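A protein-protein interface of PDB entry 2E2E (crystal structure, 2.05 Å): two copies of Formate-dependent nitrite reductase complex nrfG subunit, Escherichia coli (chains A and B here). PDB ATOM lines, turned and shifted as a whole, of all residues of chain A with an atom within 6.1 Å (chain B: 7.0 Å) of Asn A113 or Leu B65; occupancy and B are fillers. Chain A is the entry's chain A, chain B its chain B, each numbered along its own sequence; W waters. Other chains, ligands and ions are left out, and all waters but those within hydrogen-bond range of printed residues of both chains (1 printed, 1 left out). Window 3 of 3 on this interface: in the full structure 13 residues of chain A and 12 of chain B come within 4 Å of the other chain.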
ATOM      1  N   LEU A 108      15.199 -22.022  18.433  1.00  0.00           N
ATOM      2  CA  LEU A 108      16.419 -22.734  18.756  1.00  0.00           C
ATOM      3  C   LEU A 108      16.844 -23.704  17.677  1.00  0.00           C
ATOM      4  O   LEU A 108      17.934 -24.292  17.761  1.00  0.00           O
ATOM      5  CB  LEU A 108      16.300 -23.438  20.102  1.00  0.00           C
ATOM      6  CG  LEU A 108      16.270 -22.623  21.396  1.00  0.00           C
ATOM      7  CD1 LEU A 108      15.996 -23.573  22.530  1.00  0.00           C
ATOM      8  CD2 LEU A 108      17.568 -21.934  21.671  1.00  0.00           C
ATOM      9  N   ASP A 111      18.924 -21.280  15.562  1.00  0.00           N
ATOM     10  CA  ASP A 111      20.064 -20.726  16.290  1.00  0.00           C
ATOM     11  C   ASP A 111      20.054 -21.323  17.691  1.00  0.00           C
ATOM     12  O   ASP A 111      19.329 -20.868  18.595  1.00  0.00           O
ATOM     13  CB  ASP A 111      20.002 -19.181  16.334  1.00  0.00           C
ATOM     14  CG  ASP A 111      21.160 -18.534  17.145  1.00  0.00           C
ATOM     15  OD1 ASP A 111      22.125 -19.226  17.547  1.00  0.00           O
ATOM     16  OD2 ASP A 111      21.100 -17.289  17.370  1.00  0.00           O
ATOM     17  N   SER A 112      20.890 -22.329  17.879  1.00  0.00           N
ATOM     18  CA  SER A 112      20.949 -23.064  19.131  1.00  0.00           C
ATOM     19  C   SER A 112      21.417 -22.207  20.306  1.00  0.00           C
ATOM     20  O   SER A 112      21.283 -22.621  21.465  1.00  0.00           O
ATOM     21  CB  SER A 112      21.841 -24.295  18.962  1.00  0.00           C
ATOM     22  OG  SER A 112      23.034 -23.952  18.294  1.00  0.00           O
ATOM     23  N   ASN A 113      21.949 -21.016  20.015  1.00  0.00           N
ATOM     24  CA  ASN A 113      22.425 -20.100  21.052  1.00  0.00           C
ATOM     25  C   ASN A 113      21.648 -18.797  21.155  1.00  0.00           C
ATOM     26  O   ASN A 113      22.161 -17.808  21.668  1.00  0.00           O
ATOM     27  CB  ASN A 113      23.905 -19.769  20.840  1.00  0.00           C
ATOM     28  CG  ASN A 113      24.794 -21.004  20.876  1.00  0.00           C
ATOM     29  OD1 ASN A 113      24.602 -21.891  21.700  1.00  0.00           O
ATOM     30  ND2 ASN A 113      25.763 -21.055  19.996  1.00  0.00           N
ATOM     31  N   GLU A 114      20.418 -18.791  20.661  1.00  0.00           N
ATOM     32  CA  GLU A 114      19.561 -17.619  20.726  1.00  0.00           C
ATOM     33  C   GLU A 114      19.250 -17.357  22.188  1.00  0.00           C
ATOM     34  O   GLU A 114      18.545 -18.133  22.824  1.00  0.00           O
ATOM     35  CB  GLU A 114      18.282 -17.844  19.925  1.00  0.00           C
ATOM     36  CG  GLU A 114      17.760 -16.597  19.189  1.00  0.00           C
ATOM     37  CD  GLU A 114      17.338 -15.474  20.114  1.00  0.00           C
ATOM     38  OE1 GLU A 114      16.867 -15.773  21.212  1.00  0.00           O
ATOM     39  OE2 GLU A 114      17.454 -14.290  19.756  1.00  0.00           O
ATOM     40  N   ILE A 115      19.791 -16.262  22.708  1.00  0.00           N
ATOM     41  CA  ILE A 115      19.859 -15.994  24.153  1.00  0.00           C
ATOM     42  C   ILE A 115      18.477 -15.632  24.717  1.00  0.00           C
ATOM     43  O   ILE A 115      18.100 -16.065  25.798  1.00  0.00           O
ATOM     44  CB  ILE A 115      20.935 -14.920  24.429  1.00  0.00           C
ATOM     45  CG1 ILE A 115      22.325 -15.529  24.180  1.00  0.00           C
ATOM     46  CG2 ILE A 115      20.918 -14.455  25.870  1.00  0.00           C
ATOM     47  CD1 ILE A 115      23.441 -14.543  24.132  1.00  0.00           C
ATOM     48  N   THR A 116      17.698 -14.895  23.934  1.00  0.00           N
ATOM     49  CA  THR A 116      16.361 -14.544  24.311  1.00  0.00           C
ATOM     50  C   THR A 116      15.555 -15.825  24.576  1.00  0.00           C
ATOM     51  O   THR A 116      14.890 -15.924  25.602  1.00  0.00           O
ATOM     52  CB  THR A 116      15.687 -13.644  23.242  1.00  0.00           C
ATOM     53  OG1 THR A 116      16.456 -12.444  23.061  1.00  0.00           O
ATOM     54  CG2 THR A 116      14.263 -13.288  23.669  1.00  0.00           C
ATOM     55  N   LEU A 118      16.864 -18.966  25.183  1.00  0.00           N
ATOM     56  CA  LEU A 118      17.526 -19.641  26.299  1.00  0.00           C
ATOM     57  C   LEU A 118      17.170 -19.008  27.626  1.00  0.00           C
ATOM     58  O   LEU A 118      17.015 -19.700  28.618  1.00  0.00           O
ATOM     59  CB  LEU A 118      19.047 -19.628  26.146  1.00  0.00           C
ATOM     60  CG  LEU A 118      19.627 -20.507  25.018  1.00  0.00           C
ATOM     61  CD1 LEU A 118      21.123 -20.274  24.920  1.00  0.00           C
ATOM     62  CD2 LEU A 118      19.318 -21.988  25.217  1.00  0.00           C
ATOM     63  N   LYS A 140      24.994 -22.466  30.104  1.00  0.00           N
ATOM     64  CA  LYS A 140      25.145 -22.460  28.644  1.00  0.00           C
ATOM     65  C   LYS A 140      25.260 -21.028  28.151  1.00  0.00           C
ATOM     66  O   LYS A 140      26.185 -20.729  27.382  1.00  0.00           O
ATOM     67  CB  LYS A 140      24.003 -23.184  27.931  1.00  0.00           C
ATOM     68  CG  LYS A 140      24.161 -23.281  26.391  1.00  0.00           C
ATOM     69  CD  LYS A 140      22.874 -23.749  25.718  1.00  0.00           C
ATOM     70  CE  LYS A 140      22.977 -23.841  24.174  1.00  0.00           C
ATOM     71  NZ  LYS A 140      23.993 -24.856  23.731  1.00  0.00           N
ATOM     72  N   ASP A 143      28.500 -19.450  29.267  1.00  0.00           N
ATOM     73  CA  ASP A 143      29.560 -20.023  28.441  1.00  0.00           C
ATOM     74  C   ASP A 143      29.674 -19.317  27.095  1.00  0.00           C
ATOM     75  O   ASP A 143      30.694 -19.432  26.420  1.00  0.00           O
ATOM     76  CB  ASP A 143      29.310 -21.515  28.184  1.00  0.00           C
ATOM     77  CG  ASP A 143      29.690 -22.395  29.365  1.00  0.00           C
ATOM     78  OD1 ASP A 143      29.097 -23.488  29.494  1.00  0.00           O
ATOM     79  OD2 ASP A 143      30.564 -22.000  30.157  1.00  0.00           O
ATOM     80  N   LEU A 144      28.625 -18.598  26.700  1.00  0.00           N
ATOM     81  CA  LEU A 144      28.655 -17.892  25.424  1.00  0.00           C
ATOM     82  C   LEU A 144      29.524 -16.629  25.439  1.00  0.00           C
ATOM     83  O   LEU A 144      29.855 -16.103  24.375  1.00  0.00           O
ATOM     84  CB  LEU A 144      27.239 -17.588  24.922  1.00  0.00           C
ATOM     85  CG  LEU A 144      26.334 -18.806  24.670  1.00  0.00           C
ATOM     86  CD1 LEU A 144      24.920 -18.370  24.362  1.00  0.00           C
ATOM     87  CD2 LEU A 144      26.898 -19.723  23.564  1.00  0.00           C
ATOM     88  N   TRP B  47      41.157 -17.447  15.182  1.00  0.00           N
ATOM     89  CA  TRP B  47      39.739 -17.550  15.502  1.00  0.00           C
ATOM     90  C   TRP B  47      38.889 -17.070  14.326  1.00  0.00           C
ATOM     91  O   TRP B  47      37.758 -17.533  14.121  1.00  0.00           O
ATOM     92  CB  TRP B  47      39.427 -16.731  16.733  1.00  0.00           C
ATOM     93  CG  TRP B  47      39.874 -17.376  18.005  1.00  0.00           C
ATOM     94  CD1 TRP B  47      41.040 -17.141  18.683  1.00  0.00           C
ATOM     95  CD2 TRP B  47      39.172 -18.373  18.747  1.00  0.00           C
ATOM     96  NE1 TRP B  47      41.099 -17.925  19.809  1.00  0.00           N
ATOM     97  CE2 TRP B  47      39.962 -18.687  19.878  1.00  0.00           C
ATOM     98  CE3 TRP B  47      37.934 -19.017  18.583  1.00  0.00           C
ATOM     99  CZ2 TRP B  47      39.564 -19.627  20.832  1.00  0.00           C
ATOM    100  CZ3 TRP B  47      37.539 -19.949  19.527  1.00  0.00           C
ATOM    101  CH2 TRP B  47      38.355 -20.249  20.640  1.00  0.00           C
ATOM    102  N   LEU B  50      38.633 -19.905  11.885  1.00  0.00           N
ATOM    103  CA  LEU B  50      37.587 -20.783  12.386  1.00  0.00           C
ATOM    104  C   LEU B  50      36.207 -20.204  12.038  1.00  0.00           C
ATOM    105  O   LEU B  50      35.335 -20.919  11.564  1.00  0.00           O
ATOM    106  CB  LEU B  50      37.711 -20.954  13.908  1.00  0.00           C
ATOM    107  CG  LEU B  50      37.609 -22.319  14.610  1.00  0.00           C
ATOM    108  CD1 LEU B  50      37.023 -22.155  16.026  1.00  0.00           C
ATOM    109  CD2 LEU B  50      36.848 -23.379  13.829  1.00  0.00           C
ATOM    110  N   GLY B  51      36.013 -18.908  12.262  1.00  0.00           N
ATOM    111  CA  GLY B  51      34.746 -18.254  11.919  1.00  0.00           C
ATOM    112  C   GLY B  51      34.443 -18.435  10.450  1.00  0.00           C
ATOM    113  O   GLY B  51      33.305 -18.784  10.064  1.00  0.00           O
ATOM    114  N   TYR B  54      33.341 -22.163   9.603  1.00  0.00           N
ATOM    115  CA  TYR B  54      31.960 -22.349   9.998  1.00  0.00           C
ATOM    116  C   TYR B  54      30.966 -21.604   9.106  1.00  0.00           C
ATOM    117  O   TYR B  54      29.868 -22.117   8.818  1.00  0.00           O
ATOM    118  CB  TYR B  54      31.791 -21.888  11.420  1.00  0.00           C
ATOM    119  CG  TYR B  54      32.287 -22.867  12.451  1.00  0.00           C
ATOM    120  CD1 TYR B  54      33.126 -22.441  13.467  1.00  0.00           C
ATOM    121  CD2 TYR B  54      31.899 -24.209  12.425  1.00  0.00           C
ATOM    122  CE1 TYR B  54      33.561 -23.301  14.442  1.00  0.00           C
ATOM    123  CE2 TYR B  54      32.343 -25.103  13.419  1.00  0.00           C
ATOM    124  CZ  TYR B  54      33.187 -24.630  14.413  1.00  0.00           C
ATOM    125  OH  TYR B  54      33.675 -25.467  15.396  1.00  0.00           O
ATOM    126  N   ASP B  59      27.295 -22.772   9.409  1.00  0.00           N
ATOM    127  CA  ASP B  59      27.047 -22.999  10.818  1.00  0.00           C
ATOM    128  C   ASP B  59      27.158 -21.646  11.458  1.00  0.00           C
ATOM    129  O   ASP B  59      28.204 -21.291  12.024  1.00  0.00           O
ATOM    130  CB  ASP B  59      28.093 -23.947  11.400  1.00  0.00           C
ATOM    131  CG  ASP B  59      27.697 -24.522  12.768  1.00  0.00           C
ATOM    132  OD1 ASP B  59      28.435 -25.418  13.240  1.00  0.00           O
ATOM    133  OD2 ASP B  59      26.669 -24.107  13.374  1.00  0.00           O
ATOM    134  N   TYR B  60      26.089 -20.874  11.351  1.00  0.00           N
ATOM    135  CA  TYR B  60      26.128 -19.467  11.739  1.00  0.00           C
ATOM    136  C   TYR B  60      26.402 -19.239  13.250  1.00  0.00           C
ATOM    137  O   TYR B  60      27.189 -18.355  13.626  1.00  0.00           O
ATOM    138  CB  TYR B  60      24.867 -18.762  11.267  1.00  0.00           C
ATOM    139  CG  TYR B  60      24.613 -18.913   9.785  1.00  0.00           C
ATOM    140  CD1 TYR B  60      23.392 -19.377   9.320  1.00  0.00           C
ATOM    141  CD2 TYR B  60      25.604 -18.607   8.844  1.00  0.00           C
ATOM    142  CE1 TYR B  60      23.157 -19.514   7.952  1.00  0.00           C
ATOM    143  CE2 TYR B  60      25.369 -18.741   7.496  1.00  0.00           C
ATOM    144  CZ  TYR B  60      24.155 -19.194   7.063  1.00  0.00           C
ATOM    145  OH  TYR B  60      23.931 -19.333   5.731  1.00  0.00           O
ATOM    146  N   SER B  61      25.785 -20.067  14.094  1.00  0.00           N
ATOM    147  CA  SER B  61      26.013 -20.023  15.545  1.00  0.00           C
ATOM    148  C   SER B  61      27.473 -20.180  15.901  1.00  0.00           C
ATOM    149  O   SER B  61      28.020 -19.374  16.650  1.00  0.00           O
ATOM    150  CB  SER B  61      25.235 -21.133  16.254  1.00  0.00           C
ATOM    151  OG  SER B  61      23.871 -21.041  15.951  1.00  0.00           O
ATOM    152  N   ASN B  62      28.103 -21.222  15.365  1.00  0.00           N
ATOM    153  CA  ASN B  62      29.523 -21.481  15.625  1.00  0.00           C
ATOM    154  C   ASN B  62      30.435 -20.455  14.959  1.00  0.00           C
ATOM    155  O   ASN B  62      31.497 -20.109  15.490  1.00  0.00           O
ATOM    156  CB  ASN B  62      29.899 -22.896  15.206  1.00  0.00           C
ATOM    157  CG  ASN B  62      29.444 -23.947  16.221  1.00  0.00           C
ATOM    158  OD1 ASN B  62      29.608 -23.777  17.431  1.00  0.00           O
ATOM    159  ND2 ASN B  62      28.846 -25.034  15.723  1.00  0.00           N
ATOM    160  N   SER B  63      30.041 -19.996  13.781  1.00  0.00           N
ATOM    161  CA  SER B  63      30.763 -18.910  13.133  1.00  0.00           C
ATOM    162  C   SER B  63      30.783 -17.670  14.027  1.00  0.00           C
ATOM    163  O   SER B  63      31.839 -17.076  14.254  1.00  0.00           O
ATOM    164  CB  SER B  63      30.149 -18.561  11.775  1.00  0.00           C
ATOM    165  OG  SER B  63      31.080 -17.791  11.047  1.00  0.00           O
ATOM    166  N   LEU B  64      29.615 -17.288  14.528  1.00  0.00           N
ATOM    167  CA  LEU B  64      29.504 -16.099  15.382  1.00  0.00           C
ATOM    168  C   LEU B  64      30.376 -16.192  16.616  1.00  0.00           C
ATOM    169  O   LEU B  64      31.020 -15.196  17.002  1.00  0.00           O
ATOM    170  CB  LEU B  64      28.048 -15.834  15.803  1.00  0.00           C
ATOM    171  CG  LEU B  64      27.135 -15.266  14.721  1.00  0.00           C
ATOM    172  CD1 LEU B  64      25.655 -15.292  15.186  1.00  0.00           C
ATOM    173  CD2 LEU B  64      27.566 -13.841  14.289  1.00  0.00           C
ATOM    174  N   LEU B  65      30.388 -17.372  17.244  1.00  0.00           N
ATOM    175  CA  LEU B  65      31.205 -17.613  18.424  1.00  0.00           C
ATOM    176  C   LEU B  65      32.676 -17.400  18.134  1.00  0.00           C
ATOM    177  O   LEU B  65      33.365 -16.718  18.917  1.00  0.00           O
ATOM    178  CB  LEU B  65      31.002 -19.022  18.972  1.00  0.00           C
ATOM    179  CG  LEU B  65      29.668 -19.304  19.630  1.00  0.00           C
ATOM    180  CD1 LEU B  65      29.564 -20.790  19.918  1.00  0.00           C
ATOM    181  CD2 LEU B  65      29.590 -18.516  20.917  1.00  0.00           C
ATOM    182  N   ALA B  66      33.147 -17.963  17.013  1.00  0.00           N
ATOM    183  CA  ALA B  66      34.561 -17.865  16.632  1.00  0.00           C
ATOM    184  C   ALA B  66      34.955 -16.439  16.288  1.00  0.00           C
ATOM    185  O   ALA B  66      35.994 -15.964  16.723  1.00  0.00           O
ATOM    186  CB  ALA B  66      34.889 -18.804  15.491  1.00  0.00           C
ATOM    187  N   TYR B  67      34.114 -15.753  15.522  1.00  0.00           N
ATOM    188  CA  TYR B  67      34.367 -14.356  15.183  1.00  0.00           C
ATOM    189  C   TYR B  67      34.338 -13.406  16.393  1.00  0.00           C
ATOM    190  O   TYR B  67      35.096 -12.430  16.459  1.00  0.00           O
ATOM    191  CB  TYR B  67      33.415 -13.878  14.103  1.00  0.00           C
ATOM    192  CG  TYR B  67      33.879 -14.189  12.682  1.00  0.00           C
ATOM    193  CD1 TYR B  67      33.059 -14.887  11.793  1.00  0.00           C
ATOM    194  CD2 TYR B  67      35.148 -13.806  12.243  1.00  0.00           C
ATOM    195  CE1 TYR B  67      33.482 -15.174  10.497  1.00  0.00           C
ATOM    196  CE2 TYR B  67      35.587 -14.110  10.948  1.00  0.00           C
ATOM    197  CZ  TYR B  67      34.751 -14.782  10.090  1.00  0.00           C
ATOM    198  OH  TYR B  67      35.196 -15.051   8.830  1.00  0.00           O
ATOM    199  N   ARG B  68      33.448 -13.694  17.328  1.00  0.00           N
ATOM    200  CA  ARG B  68      33.306 -12.928  18.544  1.00  0.00           C
ATOM    201  C   ARG B  68      34.605 -12.976  19.339  1.00  0.00           C
ATOM    202  O   ARG B  68      35.081 -11.947  19.832  1.00  0.00           O
ATOM    203  CB  ARG B  68      32.141 -13.484  19.370  1.00  0.00           C
ATOM    204  CG  ARG B  68      31.991 -12.856  20.769  1.00  0.00           C
ATOM    205  CD  ARG B  68      30.922 -13.539  21.638  1.00  0.00           C
ATOM    206  NE  ARG B  68      29.671 -13.683  20.905  1.00  0.00           N
ATOM    207  CZ  ARG B  68      28.689 -14.518  21.229  1.00  0.00           C
ATOM    208  NH1 ARG B  68      28.790 -15.293  22.297  1.00  0.00           N
ATOM    209  NH2 ARG B  68      27.605 -14.575  20.474  1.00  0.00           N
ATOM    210  N   GLN B  69      35.169 -14.176  19.453  1.00  0.00           N
ATOM    211  CA  GLN B  69      36.430 -14.374  20.134  1.00  0.00           C
ATOM    212  C   GLN B  69      37.580 -13.638  19.432  1.00  0.00           C
ATOM    213  O   GLN B  69      38.341 -12.916  20.073  1.00  0.00           O
ATOM    214  CB  GLN B  69      36.732 -15.868  20.273  1.00  0.00           C
ATOM    215  CG  GLN B  69      38.000 -16.173  21.047  1.00  0.00           C
ATOM    216  CD  GLN B  69      37.880 -15.947  22.550  1.00  0.00           C
ATOM    217  OE1 GLN B  69      36.834 -16.144  23.130  1.00  0.00           O
ATOM    218  NE2 GLN B  69      38.978 -15.555  23.180  1.00  0.00           N
ATOM    219  N   ALA B  70      37.692 -13.815  18.112  1.00  0.00           N
ATOM    220  CA  ALA B  70      38.636 -13.053  17.308  1.00  0.00           C
ATOM    221  C   ALA B  70      38.599 -11.573  17.672  1.00  0.00           C
ATOM    222  O   ALA B  70      39.644 -10.976  17.920  1.00  0.00           O
ATOM    223  CB  ALA B  70      38.354 -13.256  15.796  1.00  0.00           C
ATOM    224  N   GLN B  72      37.179 -10.029  20.361  1.00  0.00           N
ATOM    225  CA  GLN B  72      37.523  -9.822  21.768  1.00  0.00           C
ATOM    226  C   GLN B  72      39.017  -9.561  21.924  1.00  0.00           C
ATOM    227  O   GLN B  72      39.444  -8.640  22.639  1.00  0.00           O
ATOM    228  CB  GLN B  72      37.145 -11.075  22.552  1.00  0.00           C
ATOM    229  CG  GLN B  72      36.976 -10.873  24.030  1.00  0.00           C
ATOM    230  CD  GLN B  72      35.910 -11.794  24.579  1.00  0.00           C
ATOM    231  OE1 GLN B  72      35.946 -12.172  25.753  1.00  0.00           O
ATOM    232  NE2 GLN B  72      34.938 -12.171  23.718  1.00  0.00           N
ATOM    233  N   LEU B  84      31.426 -10.490  10.994  1.00  0.00           N
ATOM    234  CA  LEU B  84      30.273 -10.588  11.879  1.00  0.00           C
ATOM    235  C   LEU B  84      28.981 -10.199  11.176  1.00  0.00           C
ATOM    236  O   LEU B  84      27.987 -10.931  11.256  1.00  0.00           O
ATOM    237  CB  LEU B  84      30.480  -9.690  13.107  1.00  0.00           C
ATOM    238  CG  LEU B  84      30.812 -10.288  14.482  1.00  0.00           C
ATOM    239  CD1 LEU B  84      31.059 -11.793  14.490  1.00  0.00           C
ATOM    240  CD2 LEU B  84      31.961  -9.538  15.160  1.00  0.00           C
ATOM    241  N   VAL B  87      27.927 -12.820   8.769  1.00  0.00           N
ATOM    242  CA  VAL B  87      27.307 -13.984   9.468  1.00  0.00           C
ATOM    243  C   VAL B  87      25.870 -13.692   9.930  1.00  0.00           C
ATOM    244  O   VAL B  87      24.934 -14.479   9.673  1.00  0.00           O
ATOM    245  CB  VAL B  87      28.177 -14.468  10.626  1.00  0.00           C
ATOM    246  CG1 VAL B  87      27.609 -15.763  11.280  1.00  0.00           C
ATOM    247  CG2 VAL B  87      29.575 -14.717  10.138  1.00  0.00           C
HETATM  248  O   HOH W   1      26.340 -18.054  18.646  1.00  0.00           O
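Hydrophobic or aromatic side chains of chain B that line the printed part of chain A: Leu B65.
Printed residues of chain A that touch a printed residue of chain B: Asp A111, Ser A112, Asn A113 and Leu A144.
Among the printed residues, 6 pairs touch across the chains.
Among the printed residues, no Asp or Glu carboxylate lies within 4 Å of a Lys or Arg side-chain nitrogen of the other chain.
Water W1 bridges the backbone carbonyl oxygen (O) of Ser B61 (2.9 Å) and the side-chain amide nitrogen (ND2) of Asn A113 (3.3 Å).
The side-chain carboxylate of Asp A111 sits at hydrogen-bond distance from the side-chain hydroxyl of Ser B61 (3.0 Å).
O of Leu A144 sits at hydrogen-bond distance from NH1 of Arg B68 (2.5 Å).
No position is printed for both chains.
Of the 6 pairs that touch across the chains among the printed residues, none has its exchanged pair printed and touching as well.
Among the printed residues, merely in contact across the chains: Ser A112 with Ser B61 (3.8 Å), Asn A113 with Ser B61 (3.8 Å), Asn A113 with Leu B65 (3.8 Å) and Leu A144 with Leu B65 (3.96 Å).
Asn A113 touches just these residues of chain B: Ser B61 and Leu B65.
Thr A116 touches none of the printed residues of chain B.
Leu B50 touches none of the printed residues of chain A.
Of the printed residues of chain A, Ser B61 touches Asp A111 (3.0 Å), Ser A112 (3.8 Å) and Asn A113 (3.8 Å).
Leu B65 touches just these residues of chain A: Asn A113 (3.8 Å) and Leu A144 (3.96 Å).
Printed residues of chain A within 4 Å of Arg B68: Leu A144.
The nearest residue of chain B that does not touch Asn A113 is Asn B62 (5.2 Å).
The nearest printed residue of chain B that does not touch Leu A144 is Gln B72 (6.5 Å).
The backbone NH (N) of Asn A113 lies close to the side-chain carboxylate (OD1) of Asp A111, at 3.1 Å.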
